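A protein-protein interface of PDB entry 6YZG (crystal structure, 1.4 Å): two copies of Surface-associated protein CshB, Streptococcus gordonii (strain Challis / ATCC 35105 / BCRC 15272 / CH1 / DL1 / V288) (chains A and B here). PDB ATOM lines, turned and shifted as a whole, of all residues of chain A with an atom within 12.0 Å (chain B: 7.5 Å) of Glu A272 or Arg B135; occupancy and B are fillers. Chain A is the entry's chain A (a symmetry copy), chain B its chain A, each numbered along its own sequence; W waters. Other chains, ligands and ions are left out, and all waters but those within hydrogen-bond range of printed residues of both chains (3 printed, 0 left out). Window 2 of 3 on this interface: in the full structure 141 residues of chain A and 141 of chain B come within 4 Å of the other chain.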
ATOM      1  N   THR A 240     -17.896 -14.312 -26.907  1.00  0.00           N
ATOM      2  CA  THR A 240     -18.683 -13.579 -25.875  1.00  0.00           C
ATOM      3  C   THR A 240     -19.973 -14.348 -25.644  1.00  0.00           C
ATOM      4  O   THR A 240     -20.580 -14.840 -26.630  1.00  0.00           O
ATOM      5  CB  THR A 240     -18.896 -12.112 -26.266  1.00  0.00           C
ATOM      6  OG1 THR A 240     -19.650 -11.486 -25.212  1.00  0.00           O
ATOM      7  CG2 THR A 240     -19.694 -11.941 -27.550  1.00  0.00           C
ATOM      8  N   ARG A 241     -20.381 -14.478 -24.386  1.00  0.00           N
ATOM      9  CA  ARG A 241     -21.626 -15.207 -24.049  1.00  0.00           C
ATOM     10  C   ARG A 241     -22.641 -14.241 -23.435  1.00  0.00           C
ATOM     11  O   ARG A 241     -22.246 -13.328 -22.788  1.00  0.00           O
ATOM     12  CB  ARG A 241     -21.302 -16.332 -23.064  1.00  0.00           C
ATOM     13  CG  ARG A 241     -22.476 -17.244 -22.734  1.00  0.00           C
ATOM     14  CD  ARG A 241     -22.126 -18.498 -21.941  1.00  0.00           C
ATOM     15  NE  ARG A 241     -21.437 -19.345 -22.874  1.00  0.00           N
ATOM     16  CZ  ARG A 241     -20.685 -20.389 -22.569  1.00  0.00           C
ATOM     17  NH1 ARG A 241     -20.469 -20.750 -21.309  1.00  0.00           N
ATOM     18  NH2 ARG A 241     -20.099 -21.046 -23.551  1.00  0.00           N
ATOM     19  N   GLY A 242     -23.925 -14.493 -23.697  1.00  0.00           N
ATOM     20  CA  GLY A 242     -24.972 -13.647 -23.112  1.00  0.00           C
ATOM     21  C   GLY A 242     -25.008 -12.258 -23.677  1.00  0.00           C
ATOM     22  O   GLY A 242     -25.421 -11.320 -22.976  1.00  0.00           O
ATOM     23  N   ALA A 243     -24.506 -12.032 -24.894  1.00  0.00           N
ATOM     24  CA  ALA A 243     -24.625 -10.732 -25.565  1.00  0.00           C
ATOM     25  C   ALA A 243     -26.023 -10.575 -26.156  1.00  0.00           C
ATOM     26  O   ALA A 243     -26.493 -11.518 -26.817  1.00  0.00           O
ATOM     27  CB  ALA A 243     -23.597 -10.639 -26.645  1.00  0.00           C
ATOM     28  N   SER A 244     -26.567  -9.404 -26.042  1.00  0.00           N
ATOM     29  CA  SER A 244     -27.699  -8.957 -26.877  1.00  0.00           C
ATOM     30  C   SER A 244     -27.268  -7.906 -27.884  1.00  0.00           C
ATOM     31  O   SER A 244     -28.108  -7.534 -28.717  1.00  0.00           O
ATOM     32  CB  SER A 244     -28.819  -8.451 -26.009  1.00  0.00           C
ATOM     33  OG  SER A 244     -28.465  -7.283 -25.310  1.00  0.00           O
ATOM     34  N   GLU A 245     -26.028  -7.413 -27.804  1.00  0.00           N
ATOM     35  CA  GLU A 245     -25.504  -6.409 -28.778  1.00  0.00           C
ATOM     36  C   GLU A 245     -24.037  -6.735 -29.041  1.00  0.00           C
ATOM     37  O   GLU A 245     -23.290  -6.989 -28.077  1.00  0.00           O
ATOM     38  CB  GLU A 245     -25.596  -4.978 -28.224  1.00  0.00           C
ATOM     39  CG  GLU A 245     -27.021  -4.578 -27.813  1.00  0.00           C
ATOM     40  CD  GLU A 245     -27.490  -3.134 -27.597  1.00  0.00           C
ATOM     41  OE1 GLU A 245     -27.684  -2.417 -28.608  1.00  0.00           O
ATOM     42  OE2 GLU A 245     -27.863  -2.785 -26.447  1.00  0.00           O
ATOM     43  N   VAL A 246     -23.664  -6.805 -30.311  1.00  0.00           N
ATOM     44  CA  VAL A 246     -22.246  -6.901 -30.678  1.00  0.00           C
ATOM     45  C   VAL A 246     -21.968  -5.890 -31.746  1.00  0.00           C
ATOM     46  O   VAL A 246     -22.849  -5.588 -32.575  1.00  0.00           O
ATOM     47  CB  VAL A 246     -21.856  -8.286 -31.171  1.00  0.00           C
ATOM     48  CG1 VAL A 246     -21.952  -9.303 -30.073  1.00  0.00           C
ATOM     49  CG2 VAL A 246     -22.608  -8.702 -32.365  1.00  0.00           C
ATOM     50  N   PHE A 262     -21.984 -18.767 -34.114  1.00  0.00           N
ATOM     51  CA  PHE A 262     -22.656 -19.154 -32.872  1.00  0.00           C
ATOM     52  C   PHE A 262     -22.267 -20.579 -32.543  1.00  0.00           C
ATOM     53  O   PHE A 262     -22.240 -21.438 -33.442  1.00  0.00           O
ATOM     54  CB  PHE A 262     -24.153 -18.997 -33.015  1.00  0.00           C
ATOM     55  CG  PHE A 262     -24.647 -17.588 -33.110  1.00  0.00           C
ATOM     56  CD1 PHE A 262     -24.478 -16.805 -34.256  1.00  0.00           C
ATOM     57  CD2 PHE A 262     -25.193 -16.961 -32.004  1.00  0.00           C
ATOM     58  CE1 PHE A 262     -24.868 -15.479 -34.252  1.00  0.00           C
ATOM     59  CE2 PHE A 262     -25.675 -15.662 -32.024  1.00  0.00           C
ATOM     60  CZ  PHE A 262     -25.482 -14.894 -33.158  1.00  0.00           C
ATOM     61  N   LEU A 263     -22.100 -20.843 -31.257  1.00  0.00           N
ATOM     62  CA  LEU A 263     -21.854 -22.216 -30.769  1.00  0.00           C
ATOM     63  C   LEU A 263     -23.151 -22.661 -30.076  1.00  0.00           C
ATOM     64  O   LEU A 263     -23.703 -21.889 -29.325  1.00  0.00           O
ATOM     65  CB  LEU A 263     -20.651 -22.228 -29.830  1.00  0.00           C
ATOM     66  CG  LEU A 263     -19.358 -21.639 -30.404  1.00  0.00           C
ATOM     67  CD1 LEU A 263     -18.224 -21.763 -29.411  1.00  0.00           C
ATOM     68  CD2 LEU A 263     -19.014 -22.270 -31.721  1.00  0.00           C
ATOM     69  N   VAL A 264     -23.603 -23.883 -30.355  1.00  0.00           N
ATOM     70  CA  VAL A 264     -24.880 -24.370 -29.761  1.00  0.00           C
ATOM     71  C   VAL A 264     -24.701 -25.616 -28.884  1.00  0.00           C
ATOM     72  O   VAL A 264     -25.702 -26.058 -28.343  1.00  0.00           O
ATOM     73  CB  VAL A 264     -25.869 -24.696 -30.889  1.00  0.00           C
ATOM     74  CG1 VAL A 264     -26.124 -23.487 -31.750  1.00  0.00           C
ATOM     75  CG2 VAL A 264     -25.340 -25.818 -31.740  1.00  0.00           C
ATOM     76  N   ALA A 266     -23.659 -26.203 -25.970  1.00  0.00           N
ATOM     77  CA  ALA A 266     -24.088 -26.174 -24.562  1.00  0.00           C
ATOM     78  C   ALA A 266     -25.389 -25.409 -24.339  1.00  0.00           C
ATOM     79  O   ALA A 266     -25.513 -24.743 -23.294  1.00  0.00           O
ATOM     80  CB  ALA A 266     -22.960 -25.599 -23.769  1.00  0.00           C
ATOM     81  N   VAL A 267     -26.365 -25.572 -25.234  1.00  0.00           N
ATOM     82  CA  VAL A 267     -27.690 -24.876 -25.099  1.00  0.00           C
ATOM     83  C   VAL A 267     -28.456 -25.422 -23.876  1.00  0.00           C
ATOM     84  O   VAL A 267     -29.163 -24.613 -23.234  1.00  0.00           O
ATOM     85  CB  VAL A 267     -28.562 -24.940 -26.377  1.00  0.00           C
ATOM     86  CG1 VAL A 267     -28.945 -26.353 -26.792  1.00  0.00           C
ATOM     87  CG2 VAL A 267     -29.836 -24.129 -26.205  1.00  0.00           C
ATOM     88  N   SER A 268     -28.328 -26.720 -23.548  1.00  0.00           N
ATOM     89  CA  SER A 268     -29.104 -27.407 -22.469  1.00  0.00           C
ATOM     90  C   SER A 268     -29.173 -26.547 -21.195  1.00  0.00           C
ATOM     91  O   SER A 268     -30.302 -26.250 -20.747  1.00  0.00           O
ATOM     92  CB  SER A 268     -28.527 -28.774 -22.159  1.00  0.00           C
ATOM     93  OG  SER A 268     -28.499 -29.592 -23.324  1.00  0.00           O
ATOM     94  N   ASP A 269     -28.014 -26.167 -20.637  1.00  0.00           N
ATOM     95  CA  ASP A 269     -27.873 -25.463 -19.327  1.00  0.00           C
ATOM     96  C   ASP A 269     -27.628 -23.961 -19.545  1.00  0.00           C
ATOM     97  O   ASP A 269     -27.214 -23.295 -18.572  1.00  0.00           O
ATOM     98  CB  ASP A 269     -26.745 -26.071 -18.485  1.00  0.00           C
ATOM     99  CG  ASP A 269     -27.046 -27.476 -17.981  1.00  0.00           C
ATOM    100  OD1 ASP A 269     -28.004 -27.621 -17.188  1.00  0.00           O
ATOM    101  OD2 ASP A 269     -26.325 -28.412 -18.389  1.00  0.00           O
ATOM    102  N   ALA A 270     -27.868 -23.451 -20.760  1.00  0.00           N
ATOM    103  CA  ALA A 270     -27.816 -22.010 -21.098  1.00  0.00           C
ATOM    104  C   ALA A 270     -28.931 -21.289 -20.356  1.00  0.00           C
ATOM    105  O   ALA A 270     -30.083 -21.717 -20.367  1.00  0.00           O
ATOM    106  CB  ALA A 270     -27.954 -21.784 -22.584  1.00  0.00           C
ATOM    107  N   PRO A 271     -28.633 -20.156 -19.698  1.00  0.00           N
ATOM    108  CA  PRO A 271     -29.690 -19.347 -19.102  1.00  0.00           C
ATOM    109  C   PRO A 271     -30.562 -18.684 -20.176  1.00  0.00           C
ATOM    110  O   PRO A 271     -30.191 -18.675 -21.403  1.00  0.00           O
ATOM    111  CB  PRO A 271     -28.933 -18.298 -18.265  1.00  0.00           C
ATOM    112  CG  PRO A 271     -27.575 -18.203 -18.921  1.00  0.00           C
ATOM    113  CD  PRO A 271     -27.294 -19.578 -19.500  1.00  0.00           C
ATOM    114  N   GLU A 272     -31.718 -18.181 -19.750  1.00  0.00           N
ATOM    115  CA  GLU A 272     -32.660 -17.438 -20.624  1.00  0.00           C
ATOM    116  C   GLU A 272     -31.971 -16.130 -21.041  1.00  0.00           C
ATOM    117  O   GLU A 272     -32.119 -15.704 -22.180  1.00  0.00           O
ATOM    118  CB  GLU A 272     -33.977 -17.193 -19.885  1.00  0.00           C
ATOM    119  CG  GLU A 272     -34.975 -16.397 -20.709  1.00  0.00           C
ATOM    120  CD  GLU A 272     -36.409 -16.542 -20.237  1.00  0.00           C
ATOM    121  OE1 GLU A 272     -37.285 -15.861 -20.809  1.00  0.00           O
ATOM    122  OE2 GLU A 272     -36.637 -17.324 -19.291  1.00  0.00           O
ATOM    123  N   SER A 273     -31.287 -15.495 -20.101  1.00  0.00           N
ATOM    124  CA  SER A 273     -30.702 -14.142 -20.298  1.00  0.00           C
ATOM    125  C   SER A 273     -29.625 -13.937 -19.250  1.00  0.00           C
ATOM    126  O   SER A 273     -29.733 -14.512 -18.150  1.00  0.00           O
ATOM    127  CB  SER A 273     -31.766 -13.085 -20.170  1.00  0.00           C
ATOM    128  OG  SER A 273     -31.224 -11.766 -20.305  1.00  0.00           O
ATOM    129  N   TYR A 274     -28.660 -13.058 -19.533  1.00  0.00           N
ATOM    130  CA  TYR A 274     -27.703 -12.557 -18.518  1.00  0.00           C
ATOM    131  C   TYR A 274     -28.288 -11.361 -17.742  1.00  0.00           C
ATOM    132  O   TYR A 274     -27.677 -10.952 -16.716  1.00  0.00           O
ATOM    133  CB  TYR A 274     -26.401 -12.238 -19.249  1.00  0.00           C
ATOM    134  CG  TYR A 274     -25.444 -13.394 -19.277  1.00  0.00           C
ATOM    135  CD1 TYR A 274     -25.802 -14.643 -19.772  1.00  0.00           C
ATOM    136  CD2 TYR A 274     -24.174 -13.221 -18.746  1.00  0.00           C
ATOM    137  CE1 TYR A 274     -24.885 -15.690 -19.790  1.00  0.00           C
ATOM    138  CE2 TYR A 274     -23.291 -14.277 -18.672  1.00  0.00           C
ATOM    139  CZ  TYR A 274     -23.608 -15.472 -19.275  1.00  0.00           C
ATOM    140  OH  TYR A 274     -22.603 -16.403 -19.152  1.00  0.00           O
ATOM    141  N   GLY A 275     -29.436 -10.842 -18.185  1.00  0.00           N
ATOM    142  CA  GLY A 275     -30.209  -9.784 -17.492  1.00  0.00           C
ATOM    143  C   GLY A 275     -30.009  -8.398 -18.100  1.00  0.00           C
ATOM    144  O   GLY A 275     -28.856  -8.065 -18.531  1.00  0.00           O
ATOM    145  N   GLU A 276     -31.074  -7.583 -18.087  1.00  0.00           N
ATOM    146  CA  GLU A 276     -31.054  -6.136 -18.453  1.00  0.00           C
ATOM    147  C   GLU A 276     -30.029  -5.385 -17.588  1.00  0.00           C
ATOM    148  O   GLU A 276     -29.326  -4.488 -18.139  1.00  0.00           O
ATOM    149  CB  GLU A 276     -32.471  -5.558 -18.353  1.00  0.00           C
ATOM    150  CG  GLU A 276     -32.545  -4.048 -18.108  1.00  0.00           C
ATOM    151  CD  GLU A 276     -32.658  -3.142 -19.328  1.00  0.00           C
ATOM    152  OE1 GLU A 276     -32.782  -1.908 -19.133  1.00  0.00           O
ATOM    153  OE2 GLU A 276     -32.621  -3.656 -20.466  1.00  0.00           O
ATOM    154  N   ALA A 277     -29.910  -5.712 -16.293  1.00  0.00           N
ATOM    155  CA  ALA A 277     -28.964  -5.068 -15.353  1.00  0.00           C
ATOM    156  C   ALA A 277     -27.525  -5.178 -15.895  1.00  0.00           C
ATOM    157  O   ALA A 277     -26.788  -4.154 -15.949  1.00  0.00           O
ATOM    158  CB  ALA A 277     -29.104  -5.723 -13.991  1.00  0.00           C
ATOM    159  N   PHE A 278     -27.126  -6.379 -16.301  1.00  0.00           N
ATOM    160  CA  PHE A 278     -25.799  -6.645 -16.919  1.00  0.00           C
ATOM    161  C   PHE A 278     -25.705  -5.942 -18.285  1.00  0.00           C
ATOM    162  O   PHE A 278     -24.713  -5.254 -18.596  1.00  0.00           O
ATOM    163  CB  PHE A 278     -25.605  -8.162 -17.068  1.00  0.00           C
ATOM    164  CG  PHE A 278     -24.250  -8.541 -17.600  1.00  0.00           C
ATOM    165  CD1 PHE A 278     -23.132  -8.508 -16.782  1.00  0.00           C
ATOM    166  CD2 PHE A 278     -24.095  -8.945 -18.910  1.00  0.00           C
ATOM    167  CE1 PHE A 278     -21.881  -8.852 -17.271  1.00  0.00           C
ATOM    168  CE2 PHE A 278     -22.839  -9.271 -19.401  1.00  0.00           C
ATOM    169  CZ  PHE A 278     -21.738  -9.213 -18.594  1.00  0.00           C
ATOM    170  N   HIS A 279     -26.700  -6.162 -19.141  1.00  0.00           N
ATOM    171  CA  HIS A 279     -26.647  -5.678 -20.541  1.00  0.00           C
ATOM    172  C   HIS A 279     -26.545  -4.157 -20.630  1.00  0.00           C
ATOM    173  O   HIS A 279     -25.989  -3.687 -21.666  1.00  0.00           O
ATOM    174  CB  HIS A 279     -27.854  -6.120 -21.346  1.00  0.00           C
ATOM    175  CG  HIS A 279     -27.809  -7.555 -21.720  1.00  0.00           C
ATOM    176  ND1 HIS A 279     -28.966  -8.290 -21.937  1.00  0.00           N
ATOM    177  CD2 HIS A 279     -26.759  -8.369 -21.977  1.00  0.00           C
ATOM    178  CE1 HIS A 279     -28.633  -9.525 -22.302  1.00  0.00           C
ATOM    179  NE2 HIS A 279     -27.267  -9.587 -22.361  1.00  0.00           N
ATOM    180  N   THR A 280     -27.099  -3.401 -19.667  1.00  0.00           N
ATOM    181  CA  THR A 280     -27.177  -1.914 -19.774  1.00  0.00           C
ATOM    182  C   THR A 280     -25.980  -1.203 -19.123  1.00  0.00           C
ATOM    183  O   THR A 280     -25.968   0.024 -19.168  1.00  0.00           O
ATOM    184  CB  THR A 280     -28.485  -1.364 -19.197  1.00  0.00           C
ATOM    185  OG1 THR A 280     -28.623  -1.917 -17.893  1.00  0.00           O
ATOM    186  CG2 THR A 280     -29.673  -1.734 -20.043  1.00  0.00           C
ATOM    187  N   ASP B 126     -28.247  -5.961 -32.781  1.00  0.00           N
ATOM    188  CA  ASP B 126     -29.017  -6.543 -31.665  1.00  0.00           C
ATOM    189  C   ASP B 126     -29.060  -8.036 -32.016  1.00  0.00           C
ATOM    190  O   ASP B 126     -29.251  -8.370 -33.165  1.00  0.00           O
ATOM    191  CB  ASP B 126     -30.408  -5.911 -31.543  1.00  0.00           C
ATOM    192  CG  ASP B 126     -30.454  -4.571 -30.808  1.00  0.00           C
ATOM    193  OD1 ASP B 126     -29.841  -4.442 -29.778  1.00  0.00           O
ATOM    194  OD2 ASP B 126     -31.103  -3.661 -31.299  1.00  0.00           O
ATOM    195  N   ILE B 127     -28.830  -8.875 -31.039  1.00  0.00           N
ATOM    196  CA  ILE B 127     -28.804 -10.341 -31.269  1.00  0.00           C
ATOM    197  C   ILE B 127     -29.873 -10.994 -30.412  1.00  0.00           C
ATOM    198  O   ILE B 127     -29.958 -10.656 -29.265  1.00  0.00           O
ATOM    199  CB  ILE B 127     -27.446 -10.926 -30.855  1.00  0.00           C
ATOM    200  CG1 ILE B 127     -26.300 -10.377 -31.691  1.00  0.00           C
ATOM    201  CG2 ILE B 127     -27.479 -12.446 -30.874  1.00  0.00           C
ATOM    202  CD1 ILE B 127     -25.013 -10.684 -30.985  1.00  0.00           C
ATOM    203  N   GLU B 128     -30.591 -11.931 -31.002  1.00  0.00           N
ATOM    204  CA  GLU B 128     -31.570 -12.752 -30.264  1.00  0.00           C
ATOM    205  C   GLU B 128     -31.390 -14.198 -30.715  1.00  0.00           C
ATOM    206  O   GLU B 128     -31.254 -14.443 -31.881  1.00  0.00           O
ATOM    207  CB  GLU B 128     -32.969 -12.274 -30.608  1.00  0.00           C
ATOM    208  CG  GLU B 128     -34.106 -13.201 -30.242  1.00  0.00           C
ATOM    209  CD  GLU B 128     -35.317 -12.635 -30.961  1.00  0.00           C
ATOM    210  OE1 GLU B 128     -35.622 -11.475 -30.686  1.00  0.00           O
ATOM    211  OE2 GLU B 128     -35.813 -13.273 -31.889  1.00  0.00           O
ATOM    212  N   ALA B 129     -31.300 -15.088 -29.754  1.00  0.00           N
ATOM    213  CA  ALA B 129     -31.244 -16.522 -30.052  1.00  0.00           C
ATOM    214  C   ALA B 129     -32.431 -17.176 -29.379  1.00  0.00           C
ATOM    215  O   ALA B 129     -32.733 -16.851 -28.227  1.00  0.00           O
ATOM    216  CB  ALA B 129     -29.981 -17.138 -29.533  1.00  0.00           C
ATOM    217  N   THR B 130     -33.094 -18.073 -30.091  1.00  0.00           N
ATOM    218  CA  THR B 130     -34.187 -18.889 -29.497  1.00  0.00           C
ATOM    219  C   THR B 130     -33.930 -20.359 -29.737  1.00  0.00           C
ATOM    220  O   THR B 130     -33.406 -20.770 -30.761  1.00  0.00           O
ATOM    221  CB  THR B 130     -35.552 -18.490 -30.021  1.00  0.00           C
ATOM    222  OG1 THR B 130     -35.605 -18.784 -31.434  1.00  0.00           O
ATOM    223  CG2 THR B 130     -35.872 -17.039 -29.766  1.00  0.00           C
ATOM    224  N   TYR B 131     -34.270 -21.163 -28.730  1.00  0.00           N
ATOM    225  CA  TYR B 131     -34.185 -22.624 -28.841  1.00  0.00           C
ATOM    226  C   TYR B 131     -35.579 -23.186 -28.570  1.00  0.00           C
ATOM    227  O   TYR B 131     -36.104 -22.929 -27.515  1.00  0.00           O
ATOM    228  CB  TYR B 131     -33.129 -23.275 -27.961  1.00  0.00           C
ATOM    229  CG  TYR B 131     -33.050 -24.761 -28.188  1.00  0.00           C
ATOM    230  CD1 TYR B 131     -32.751 -25.298 -29.434  1.00  0.00           C
ATOM    231  CD2 TYR B 131     -33.398 -25.641 -27.168  1.00  0.00           C
ATOM    232  CE1 TYR B 131     -32.720 -26.671 -29.653  1.00  0.00           C
ATOM    233  CE2 TYR B 131     -33.350 -27.012 -27.364  1.00  0.00           C
ATOM    234  CZ  TYR B 131     -33.042 -27.528 -28.606  1.00  0.00           C
ATOM    235  OH  TYR B 131     -33.002 -28.893 -28.809  1.00  0.00           O
ATOM    236  N   LEU B 132     -36.163 -23.773 -29.615  1.00  0.00           N
ATOM    237  CA  LEU B 132     -37.574 -24.274 -29.569  1.00  0.00           C
ATOM    238  C   LEU B 132     -38.487 -23.154 -29.096  1.00  0.00           C
ATOM    239  O   LEU B 132     -39.375 -23.419 -28.198  1.00  0.00           O
ATOM    240  CB  LEU B 132     -37.645 -25.499 -28.650  1.00  0.00           C
ATOM    241  CG  LEU B 132     -36.768 -26.685 -28.995  1.00  0.00           C
ATOM    242  CD1 LEU B 132     -36.953 -27.803 -27.961  1.00  0.00           C
ATOM    243  CD2 LEU B 132     -37.027 -27.205 -30.398  1.00  0.00           C
ATOM    244  N   GLY B 133     -38.296 -21.930 -29.599  1.00  0.00           N
ATOM    245  CA  GLY B 133     -39.141 -20.752 -29.392  1.00  0.00           C
ATOM    246  C   GLY B 133     -38.867 -19.986 -28.113  1.00  0.00           C
ATOM    247  O   GLY B 133     -39.523 -18.920 -27.974  1.00  0.00           O
ATOM    248  N   LYS B 134     -37.981 -20.490 -27.243  1.00  0.00           N
ATOM    249  CA  LYS B 134     -37.643 -19.814 -25.949  1.00  0.00           C
ATOM    250  C   LYS B 134     -36.316 -19.055 -26.144  1.00  0.00           C
ATOM    251  O   LYS B 134     -35.369 -19.672 -26.601  1.00  0.00           O
ATOM    252  CB  LYS B 134     -37.531 -20.833 -24.827  1.00  0.00           C
ATOM    253  CG  LYS B 134     -38.880 -21.519 -24.534  1.00  0.00           C
ATOM    254  CD  LYS B 134     -38.834 -22.459 -23.376  1.00  0.00           C
ATOM    255  CE  LYS B 134     -40.167 -23.147 -23.132  1.00  0.00           C
ATOM    256  NZ  LYS B 134     -40.049 -24.128 -22.023  1.00  0.00           N
ATOM    257  N   ARG B 135     -36.263 -17.846 -25.616  1.00  0.00           N
ATOM    258  CA  ARG B 135     -35.023 -17.054 -25.693  1.00  0.00           C
ATOM    259  C   ARG B 135     -33.934 -17.745 -24.876  1.00  0.00           C
ATOM    260  O   ARG B 135     -34.185 -18.222 -23.796  1.00  0.00           O
ATOM    261  CB  ARG B 135     -35.275 -15.599 -25.298  1.00  0.00           C
ATOM    262  CG  ARG B 135     -34.045 -14.717 -25.481  1.00  0.00           C
ATOM    263  CD  ARG B 135     -34.380 -13.276 -25.786  1.00  0.00           C
ATOM    264  NE  ARG B 135     -33.114 -12.573 -25.851  1.00  0.00           N
ATOM    265  CZ  ARG B 135     -32.917 -11.355 -26.291  1.00  0.00           C
ATOM    266  NH1 ARG B 135     -33.946 -10.620 -26.679  1.00  0.00           N
ATOM    267  NH2 ARG B 135     -31.690 -10.866 -26.280  1.00  0.00           N
ATOM    268  N   VAL B 136     -32.732 -17.748 -25.414  1.00  0.00           N
ATOM    269  CA  VAL B 136     -31.566 -18.342 -24.724  1.00  0.00           C
ATOM    270  C   VAL B 136     -30.369 -17.382 -24.862  1.00  0.00           C
ATOM    271  O   VAL B 136     -30.315 -16.615 -25.769  1.00  0.00           O
ATOM    272  CB  VAL B 136     -31.215 -19.746 -25.264  1.00  0.00           C
ATOM    273  CG1 VAL B 136     -32.258 -20.810 -24.920  1.00  0.00           C
ATOM    274  CG2 VAL B 136     -30.912 -19.748 -26.754  1.00  0.00           C
ATOM    275  N   ALA B 137     -29.456 -17.509 -23.926  1.00  0.00           N
ATOM    276  CA  ALA B 137     -28.197 -16.724 -23.987  1.00  0.00           C
ATOM    277  C   ALA B 137     -27.347 -17.356 -25.073  1.00  0.00           C
ATOM    278  O   ALA B 137     -26.933 -18.497 -24.946  1.00  0.00           O
ATOM    279  CB  ALA B 137     -27.482 -16.746 -22.663  1.00  0.00           C
ATOM    280  N   PRO B 138     -26.906 -16.580 -26.073  1.00  0.00           N
ATOM    281  CA  PRO B 138     -26.069 -17.162 -27.113  1.00  0.00           C
ATOM    282  C   PRO B 138     -24.579 -17.149 -26.766  1.00  0.00           C
ATOM    283  O   PRO B 138     -24.156 -16.416 -25.844  1.00  0.00           O
ATOM    284  CB  PRO B 138     -26.328 -16.170 -28.241  1.00  0.00           C
ATOM    285  CG  PRO B 138     -26.510 -14.865 -27.583  1.00  0.00           C
ATOM    286  CD  PRO B 138     -27.259 -15.174 -26.273  1.00  0.00           C
HETATM  287  O   HOH W   1     -29.116 -12.261 -26.329  1.00  0.00           O
HETATM  288  O   HOH W   2     -31.382 -13.490 -23.623  1.00  0.00           O
HETATM  289  O   HOH W   3     -23.242 -13.712 -26.886  1.00  0.00           O
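NH2 of Arg B135 is in hydrogen-bond range of O of Ile B127 (3.5 Å).
O of Ala B129 lies within hydrogen-bond range of N of Val B136, 3.0 Å away.
The backbone carbonyl oxygen of Gly A242 sits at hydrogen-bond distance from a ring nitrogen (NE2) of His A279.
Printed residues of chain B that touch a printed residue of chain A: Asp B126, Ile B127, Tyr B131, Arg B135, Val B136, Ala B137 and Pro B138.
Hydrophobic or aromatic side chains of chain B within 4 Å of the printed part of chain A: Ile B127, Tyr B131, Ala B137 and Pro B138.
Of the 25 printed residues of chain A, 12 touch a printed residue of chain B.
Hydrophobic or aromatic side chains of chain A within 4 Å of the printed part of chain B: Val A246, Phe A262, Val A267 and Tyr A274.
Glu A272 touches just these residues of chain B: Arg B135, Val B136 and Ala B137.
Arg B135 touches just these residues of chain A: Ser A244 and Glu A272.
No residue of chain A comes within 4 Å of Glu B128.
Ala B129 touches none of the printed residues of chain A.
No residue of chain A comes within 4 Å of Thr B130.
Gly B133 touches none of the printed residues of chain A.
Val B136 touches two residues of chain A.
Printed residues of chain B within 4 Å of Val A267: Tyr B131 (3.8 Å).
Printed residues of chain B within 4 Å of Thr A240: Pro B138 (3.99 Å).
Of the printed residues of chain A, Asp B126 touches Ser A244 and Glu A245.
Ser A273 touches none of the printed residues of chain B.
The nearest printed residue of chain B that does not touch Glu A272 is Ala B129 (6.2 Å).
No position is printed for both chains.
Water W2 bridges O of Glu A272 (2.7 Å) and NE of Arg B135 (3.0 Å).
Water W1 lies within hydrogen-bond range of O of Ala A243, NH2 of Arg B135 and O of Ile B127.
Water W3 lies within hydrogen-bond range of N of Ala A243 (2.9 Å), O of Thr A240 (2.9 Å), O of Pro B138 (3.0 Å) and N of Gly A242 (3.4 Å).
N of Ile B127 sits at hydrogen-bond distance from O of Ser A244, at 2.8 Å.
The backbone NH (N) of Ala B137 sits at hydrogen-bond distance from the backbone carbonyl oxygen (O) of Pro A271.
N of Gly A242 is in hydrogen-bond range of O of Pro B138 (2.9 Å).
OD1 of Asp B126 lies close to OE1 of Glu A245, at 3.2 Å.
O of Ala A243 touches CG of Pro B138, 3.4 Å away.
Ser A244 touches Asp B126.
Arg B135 touches Ser A244 (NH2 to CB, 3.8 Å).
Val A246 touches Ile B127.
Phe A262 touches Ile B127 (CE2 to CG2, 3.9 Å).
CB of Tyr B131 touches CG2 of Val A267 (3.8 Å).
Pro A271 touches Val B136 (O to CA, 3.6 Å).
C of Val B136 touches O of Glu A272, at 3.6 Å.
Glu A272 touches Ala B137 (O to N, 3.7 Å).
Ala B137 touches Tyr A274 (CB to CD1, 3.95 Å).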
